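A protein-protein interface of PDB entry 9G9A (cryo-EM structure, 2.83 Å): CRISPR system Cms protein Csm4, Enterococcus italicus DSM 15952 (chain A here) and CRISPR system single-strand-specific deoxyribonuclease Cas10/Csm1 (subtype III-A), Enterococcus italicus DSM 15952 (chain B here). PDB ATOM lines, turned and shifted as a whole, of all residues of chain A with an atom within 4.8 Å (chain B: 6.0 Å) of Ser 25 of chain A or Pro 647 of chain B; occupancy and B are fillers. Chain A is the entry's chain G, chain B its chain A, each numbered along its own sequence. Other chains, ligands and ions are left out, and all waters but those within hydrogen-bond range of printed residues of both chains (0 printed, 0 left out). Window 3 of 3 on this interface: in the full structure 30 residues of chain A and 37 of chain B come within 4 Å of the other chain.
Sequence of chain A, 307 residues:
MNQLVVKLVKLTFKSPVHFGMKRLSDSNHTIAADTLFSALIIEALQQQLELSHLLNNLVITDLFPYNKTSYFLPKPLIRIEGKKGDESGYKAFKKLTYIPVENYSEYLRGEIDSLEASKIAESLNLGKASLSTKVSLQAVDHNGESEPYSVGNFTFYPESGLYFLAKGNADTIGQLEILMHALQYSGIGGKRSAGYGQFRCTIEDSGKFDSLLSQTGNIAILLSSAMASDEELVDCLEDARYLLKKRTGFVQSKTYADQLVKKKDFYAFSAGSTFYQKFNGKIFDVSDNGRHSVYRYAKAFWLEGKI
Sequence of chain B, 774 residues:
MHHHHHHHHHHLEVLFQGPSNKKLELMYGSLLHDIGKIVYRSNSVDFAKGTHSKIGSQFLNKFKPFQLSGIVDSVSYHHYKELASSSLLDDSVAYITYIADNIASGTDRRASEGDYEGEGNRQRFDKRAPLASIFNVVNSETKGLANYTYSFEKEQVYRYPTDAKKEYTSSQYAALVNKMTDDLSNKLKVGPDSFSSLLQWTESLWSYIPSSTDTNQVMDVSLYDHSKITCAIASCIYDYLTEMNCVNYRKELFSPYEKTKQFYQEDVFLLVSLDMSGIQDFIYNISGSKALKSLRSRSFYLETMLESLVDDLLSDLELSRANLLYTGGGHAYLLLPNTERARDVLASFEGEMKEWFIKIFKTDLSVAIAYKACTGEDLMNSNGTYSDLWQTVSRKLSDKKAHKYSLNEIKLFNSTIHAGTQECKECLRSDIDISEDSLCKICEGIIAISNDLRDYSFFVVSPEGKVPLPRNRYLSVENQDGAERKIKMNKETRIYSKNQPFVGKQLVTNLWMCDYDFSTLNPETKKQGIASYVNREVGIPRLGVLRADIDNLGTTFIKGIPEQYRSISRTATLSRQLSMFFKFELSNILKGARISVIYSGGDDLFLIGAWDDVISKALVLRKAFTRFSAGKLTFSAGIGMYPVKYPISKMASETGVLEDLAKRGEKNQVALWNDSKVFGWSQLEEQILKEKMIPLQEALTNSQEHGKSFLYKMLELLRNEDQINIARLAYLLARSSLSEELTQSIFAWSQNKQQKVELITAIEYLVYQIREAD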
ATOM      1  N   ARG A  23      -8.871   4.430  13.930  1.00  0.00           N
ATOM      2  CA  ARG A  23      -8.784   5.644  13.132  1.00  0.00           C
ATOM      3  C   ARG A  23      -7.423   6.299  13.326  1.00  0.00           C
ATOM      4  O   ARG A  23      -6.730   6.063  14.318  1.00  0.00           O
ATOM      5  CB  ARG A  23      -9.898   6.633  13.497  1.00  0.00           C
ATOM      6  CG  ARG A  23     -11.290   6.095  13.234  1.00  0.00           C
ATOM      7  CD  ARG A  23     -12.343   6.824  14.044  1.00  0.00           C
ATOM      8  NE  ARG A  23     -13.658   6.222  13.861  1.00  0.00           N
ATOM      9  CZ  ARG A  23     -14.081   5.142  14.505  1.00  0.00           C
ATOM     10  NH1 ARG A  23     -13.318   4.521  15.388  1.00  0.00           N
ATOM     11  NH2 ARG A  23     -15.300   4.673  14.252  1.00  0.00           N
ATOM     12  N   LEU A  24      -7.049   7.129  12.350  1.00  0.00           N
ATOM     13  CA  LEU A  24      -5.781   7.844  12.430  1.00  0.00           C
ATOM     14  C   LEU A  24      -5.784   8.861  13.563  1.00  0.00           C
ATOM     15  O   LEU A  24      -4.723   9.184  14.108  1.00  0.00           O
ATOM     16  CB  LEU A  24      -5.482   8.524  11.093  1.00  0.00           C
ATOM     17  CG  LEU A  24      -4.105   9.158  10.886  1.00  0.00           C
ATOM     18  CD1 LEU A  24      -3.014   8.107  10.879  1.00  0.00           C
ATOM     19  CD2 LEU A  24      -4.077   9.959   9.600  1.00  0.00           C
ATOM     20  N   SER A  25      -6.959   9.374  13.932  1.00  0.00           N
ATOM     21  CA  SER A  25      -7.032  10.341  15.023  1.00  0.00           C
ATOM     22  C   SER A  25      -6.915   9.659  16.381  1.00  0.00           C
ATOM     23  O   SER A  25      -6.632  10.315  17.390  1.00  0.00           O
ATOM     24  CB  SER A  25      -8.335  11.134  14.928  1.00  0.00           C
ATOM     25  OG  SER A  25      -9.459  10.276  14.934  1.00  0.00           O
ATOM     26  N   ASP A  26      -7.137   8.348  16.429  1.00  0.00           N
ATOM     27  CA  ASP A  26      -7.010   7.616  17.682  1.00  0.00           C
ATOM     28  C   ASP A  26      -5.550   7.543  18.113  1.00  0.00           C
ATOM     29  O   ASP A  26      -4.653   7.328  17.294  1.00  0.00           O
ATOM     30  CB  ASP A  26      -7.588   6.208  17.534  1.00  0.00           C
ATOM     31  CG  ASP A  26      -9.101   6.209  17.438  1.00  0.00           C
ATOM     32  OD1 ASP A  26      -9.704   7.295  17.566  1.00  0.00           O
ATOM     33  OD2 ASP A  26      -9.689   5.127  17.235  1.00  0.00           O
ATOM     34  N   SER A  27      -5.314   7.723  19.414  1.00  0.00           N
ATOM     35  CA  SER A  27      -3.969   7.713  19.982  1.00  0.00           C
ATOM     36  C   SER A  27      -3.941   6.770  21.186  1.00  0.00           C
ATOM     37  O   SER A  27      -4.099   7.190  22.332  1.00  0.00           O
ATOM     38  CB  SER A  27      -3.534   9.124  20.376  1.00  0.00           C
ATOM     39  OG  SER A  27      -4.411   9.675  21.340  1.00  0.00           O
ATOM     40  N   LEU A 131      -3.355  15.251  19.687  1.00  0.00           N
ATOM     41  CA  LEU A 131      -3.853  15.164  18.319  1.00  0.00           C
ATOM     42  C   LEU A 131      -3.149  16.229  17.489  1.00  0.00           C
ATOM     43  O   LEU A 131      -3.351  17.429  17.709  1.00  0.00           O
ATOM     44  CB  LEU A 131      -5.367  15.351  18.280  1.00  0.00           C
ATOM     45  CG  LEU A 131      -6.057  14.970  16.974  1.00  0.00           C
ATOM     46  CD1 LEU A 131      -5.978  13.474  16.758  1.00  0.00           C
ATOM     47  CD2 LEU A 131      -7.495  15.434  16.979  1.00  0.00           C
ATOM     48  N   SER A 150      -6.149  14.675  11.054  1.00  0.00           N
ATOM     49  CA  SER A 150      -5.638  14.587  12.413  1.00  0.00           C
ATOM     50  C   SER A 150      -4.943  13.250  12.613  1.00  0.00           C
ATOM     51  O   SER A 150      -5.463  12.206  12.203  1.00  0.00           O
ATOM     52  CB  SER A 150      -6.764  14.758  13.435  1.00  0.00           C
ATOM     53  OG  SER A 150      -7.315  16.063  13.375  1.00  0.00           O
ATOM     54  N   VAL A 151      -3.765  13.288  13.232  1.00  0.00           N
ATOM     55  CA  VAL A 151      -3.017  12.095  13.609  1.00  0.00           C
ATOM     56  C   VAL A 151      -2.936  12.069  15.128  1.00  0.00           C
ATOM     57  O   VAL A 151      -2.447  13.020  15.748  1.00  0.00           O
ATOM     58  CB  VAL A 151      -1.613  12.081  12.983  1.00  0.00           C
ATOM     59  CG1 VAL A 151      -0.859  10.835  13.403  1.00  0.00           C
ATOM     60  CG2 VAL A 151      -1.704  12.161  11.472  1.00  0.00           C
ATOM     61  N   GLY A 152      -3.424  10.989  15.731  1.00  0.00           N
ATOM     62  CA  GLY A 152      -3.303  10.847  17.169  1.00  0.00           C
ATOM     63  C   GLY A 152      -1.943  10.284  17.545  1.00  0.00           C
ATOM     64  O   GLY A 152      -1.481   9.288  16.986  1.00  0.00           O
ATOM     65  N   ILE B 286     -17.608   7.274  15.824  1.00  0.00           N
ATOM     66  CA  ILE B 286     -18.035   7.396  14.437  1.00  0.00           C
ATOM     67  C   ILE B 286     -17.120   8.392  13.740  1.00  0.00           C
ATOM     68  O   ILE B 286     -16.700   9.389  14.339  1.00  0.00           O
ATOM     69  CB  ILE B 286     -19.511   7.833  14.327  1.00  0.00           C
ATOM     70  CG1 ILE B 286     -19.782   9.050  15.210  1.00  0.00           C
ATOM     71  CG2 ILE B 286     -20.432   6.690  14.704  1.00  0.00           C
ATOM     72  CD1 ILE B 286     -21.231   9.475  15.234  1.00  0.00           C
ATOM     73  N   LYS B 645     -15.086  19.895  12.762  1.00  0.00           N
ATOM     74  CA  LYS B 645     -14.381  18.836  12.051  1.00  0.00           C
ATOM     75  C   LYS B 645     -13.440  18.075  12.979  1.00  0.00           C
ATOM     76  O   LYS B 645     -12.784  17.136  12.530  1.00  0.00           O
ATOM     77  CB  LYS B 645     -13.591  19.338  10.826  1.00  0.00           C
ATOM     78  CG  LYS B 645     -14.446  20.060   9.800  1.00  0.00           C
ATOM     79  CD  LYS B 645     -13.603  20.629   8.677  1.00  0.00           C
ATOM     80  CE  LYS B 645     -14.463  21.390   7.682  1.00  0.00           C
ATOM     81  NZ  LYS B 645     -15.203  22.505   8.334  1.00  0.00           N
ATOM     82  N   TYR B 646     -13.345  18.449  14.249  1.00  0.00           N
ATOM     83  CA  TYR B 646     -12.623  17.648  15.227  1.00  0.00           C
ATOM     84  C   TYR B 646     -13.325  16.303  15.369  1.00  0.00           C
ATOM     85  O   TYR B 646     -14.560  16.254  15.354  1.00  0.00           O
ATOM     86  CB  TYR B 646     -12.585  18.380  16.567  1.00  0.00           C
ATOM     87  CG  TYR B 646     -11.432  18.031  17.481  1.00  0.00           C
ATOM     88  CD1 TYR B 646     -11.568  17.066  18.464  1.00  0.00           C
ATOM     89  CD2 TYR B 646     -10.217  18.691  17.379  1.00  0.00           C
ATOM     90  CE1 TYR B 646     -10.524  16.753  19.309  1.00  0.00           C
ATOM     91  CE2 TYR B 646      -9.166  18.385  18.219  1.00  0.00           C
ATOM     92  CZ  TYR B 646      -9.325  17.415  19.183  1.00  0.00           C
ATOM     93  OH  TYR B 646      -8.281  17.105  20.024  1.00  0.00           O
ATOM     94  N   PRO B 647     -12.589  15.198  15.483  1.00  0.00           N
ATOM     95  CA  PRO B 647     -13.245  13.888  15.585  1.00  0.00           C
ATOM     96  C   PRO B 647     -14.178  13.832  16.787  1.00  0.00           C
ATOM     97  O   PRO B 647     -13.835  14.274  17.884  1.00  0.00           O
ATOM     98  CB  PRO B 647     -12.069  12.916  15.731  1.00  0.00           C
ATOM     99  CG  PRO B 647     -10.907  13.637  15.126  1.00  0.00           C
ATOM    100  CD  PRO B 647     -11.122  15.084  15.439  1.00  0.00           C
ATOM    101  N   ILE B 648     -15.376  13.286  16.563  1.00  0.00           N
ATOM    102  CA  ILE B 648     -16.364  13.203  17.634  1.00  0.00           C
ATOM    103  C   ILE B 648     -15.891  12.247  18.719  1.00  0.00           C
ATOM    104  O   ILE B 648     -16.100  12.489  19.914  1.00  0.00           O
ATOM    105  CB  ILE B 648     -17.733  12.793  17.066  1.00  0.00           C
ATOM    106  CG1 ILE B 648     -18.231  13.847  16.078  1.00  0.00           C
ATOM    107  CG2 ILE B 648     -18.742  12.594  18.184  1.00  0.00           C
ATOM    108  CD1 ILE B 648     -19.630  13.598  15.583  1.00  0.00           C
ATOM    109  N   SER B 649     -15.243  11.149  18.324  1.00  0.00           N
ATOM    110  CA  SER B 649     -14.653  10.253  19.311  1.00  0.00           C
ATOM    111  C   SER B 649     -13.572  10.964  20.112  1.00  0.00           C
ATOM    112  O   SER B 649     -13.451  10.757  21.324  1.00  0.00           O
ATOM    113  CB  SER B 649     -14.090   9.010  18.621  1.00  0.00           C
ATOM    114  OG  SER B 649     -13.116   9.355  17.654  1.00  0.00           O
ATOM    115  N   LYS B 650     -12.784  11.818  19.454  1.00  0.00           N
ATOM    116  CA  LYS B 650     -11.756  12.569  20.168  1.00  0.00           C
ATOM    117  C   LYS B 650     -12.371  13.564  21.145  1.00  0.00           C
ATOM    118  O   LYS B 650     -11.897  13.697  22.279  1.00  0.00           O
ATOM    119  CB  LYS B 650     -10.843  13.283  19.174  1.00  0.00           C
ATOM    120  CG  LYS B 650      -9.498  12.608  18.979  1.00  0.00           C
ATOM    121  CD  LYS B 650      -8.706  12.582  20.275  1.00  0.00           C
ATOM    122  CE  LYS B 650      -7.334  11.966  20.074  1.00  0.00           C
ATOM    123  NZ  LYS B 650      -6.553  11.908  21.340  1.00  0.00           N
ATOM    124  N   MET B 651     -13.423  14.275  20.724  1.00  0.00           N
ATOM    125  CA  MET B 651     -14.106  15.189  21.636  1.00  0.00           C
ATOM    126  C   MET B 651     -14.678  14.441  22.831  1.00  0.00           C
ATOM    127  O   MET B 651     -14.530  14.878  23.978  1.00  0.00           O
ATOM    128  CB  MET B 651     -15.220  15.942  20.905  1.00  0.00           C
ATOM    129  CG  MET B 651     -14.752  16.832  19.771  1.00  0.00           C
ATOM    130  SD  MET B 651     -16.065  17.889  19.127  1.00  0.00           S
ATOM    131  CE  MET B 651     -17.297  16.673  18.682  1.00  0.00           C
ATOM    132  N   ALA B 652     -15.320  13.298  22.578  1.00  0.00           N
ATOM    133  CA  ALA B 652     -15.887  12.507  23.663  1.00  0.00           C
ATOM    134  C   ALA B 652     -14.806  12.023  24.617  1.00  0.00           C
ATOM    135  O   ALA B 652     -14.973  12.099  25.837  1.00  0.00           O
ATOM    136  CB  ALA B 652     -16.672  11.325  23.093  1.00  0.00           C
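N of Arg 23 of chain A sits at hydrogen-bond distance from OD2 of Asp 26 of chain A.
Among the printed residues, pairs that only touch across the chains: Ser 25 of chain A with Lys 650 of chain B (3.2 Å), Leu 131 of chain A with Tyr 646 of chain B (3.5 Å), Ser 25 of chain A with Pro 647 of chain B (3.6 Å), Arg 23 of chain A with Ile 286 of chain B (3.8 Å), Leu 131 of chain A with Lys 650 of chain B (3.9 Å), Leu 131 of chain A with Pro 647 of chain B (3.96 Å) and Asp 26 of chain A with Ser 649 of chain B (3.99 Å).
Printed residues of chain A that touch a printed residue of chain B: Arg 23, Ser 25, Asp 26, Ser 27 and Leu 131. Of the 9 printed residues of chain B, 5 touch a printed residue of chain A. Printed residues of chain B that touch a printed residue of chain A: Ile 286, Tyr 646, Pro 647, Ser 649 and Lys 650. Hydrophobic or aromatic side chains of chain B within 4 Å of the printed part of chain A: Tyr 646 and Pro 647. Among the printed residues, no Asp or Glu carboxylate lies within 4 Å of a Lys or Arg side-chain nitrogen of the other chain.
Ser 25 of chain A touches just these residues of chain B: Pro 647 and Lys 650. Pro 647 of chain B touches two residues of chain A. Of the printed residues of chain B, Arg 23 of chain A touches Ile 286. Printed residues of chain B within 4 Å of Leu 131 of chain A: Tyr 646, Pro 647 and Lys 650. Of the printed residues of chain B, Ser 27 of chain A touches Lys 650. Of the printed residues of chain A, Ile 286 of chain B touches Arg 23 (3.8 Å). The nearest residue of chain B that does not touch Ser 25 of chain A is Ser 649 of chain B (4.6 Å).
The side-chain hydroxyl (OG) of Ser 27 of chain A lies within hydrogen-bond range of the side-chain amino group (NZ) of Lys 650 of chain B, at 3.1 Å.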
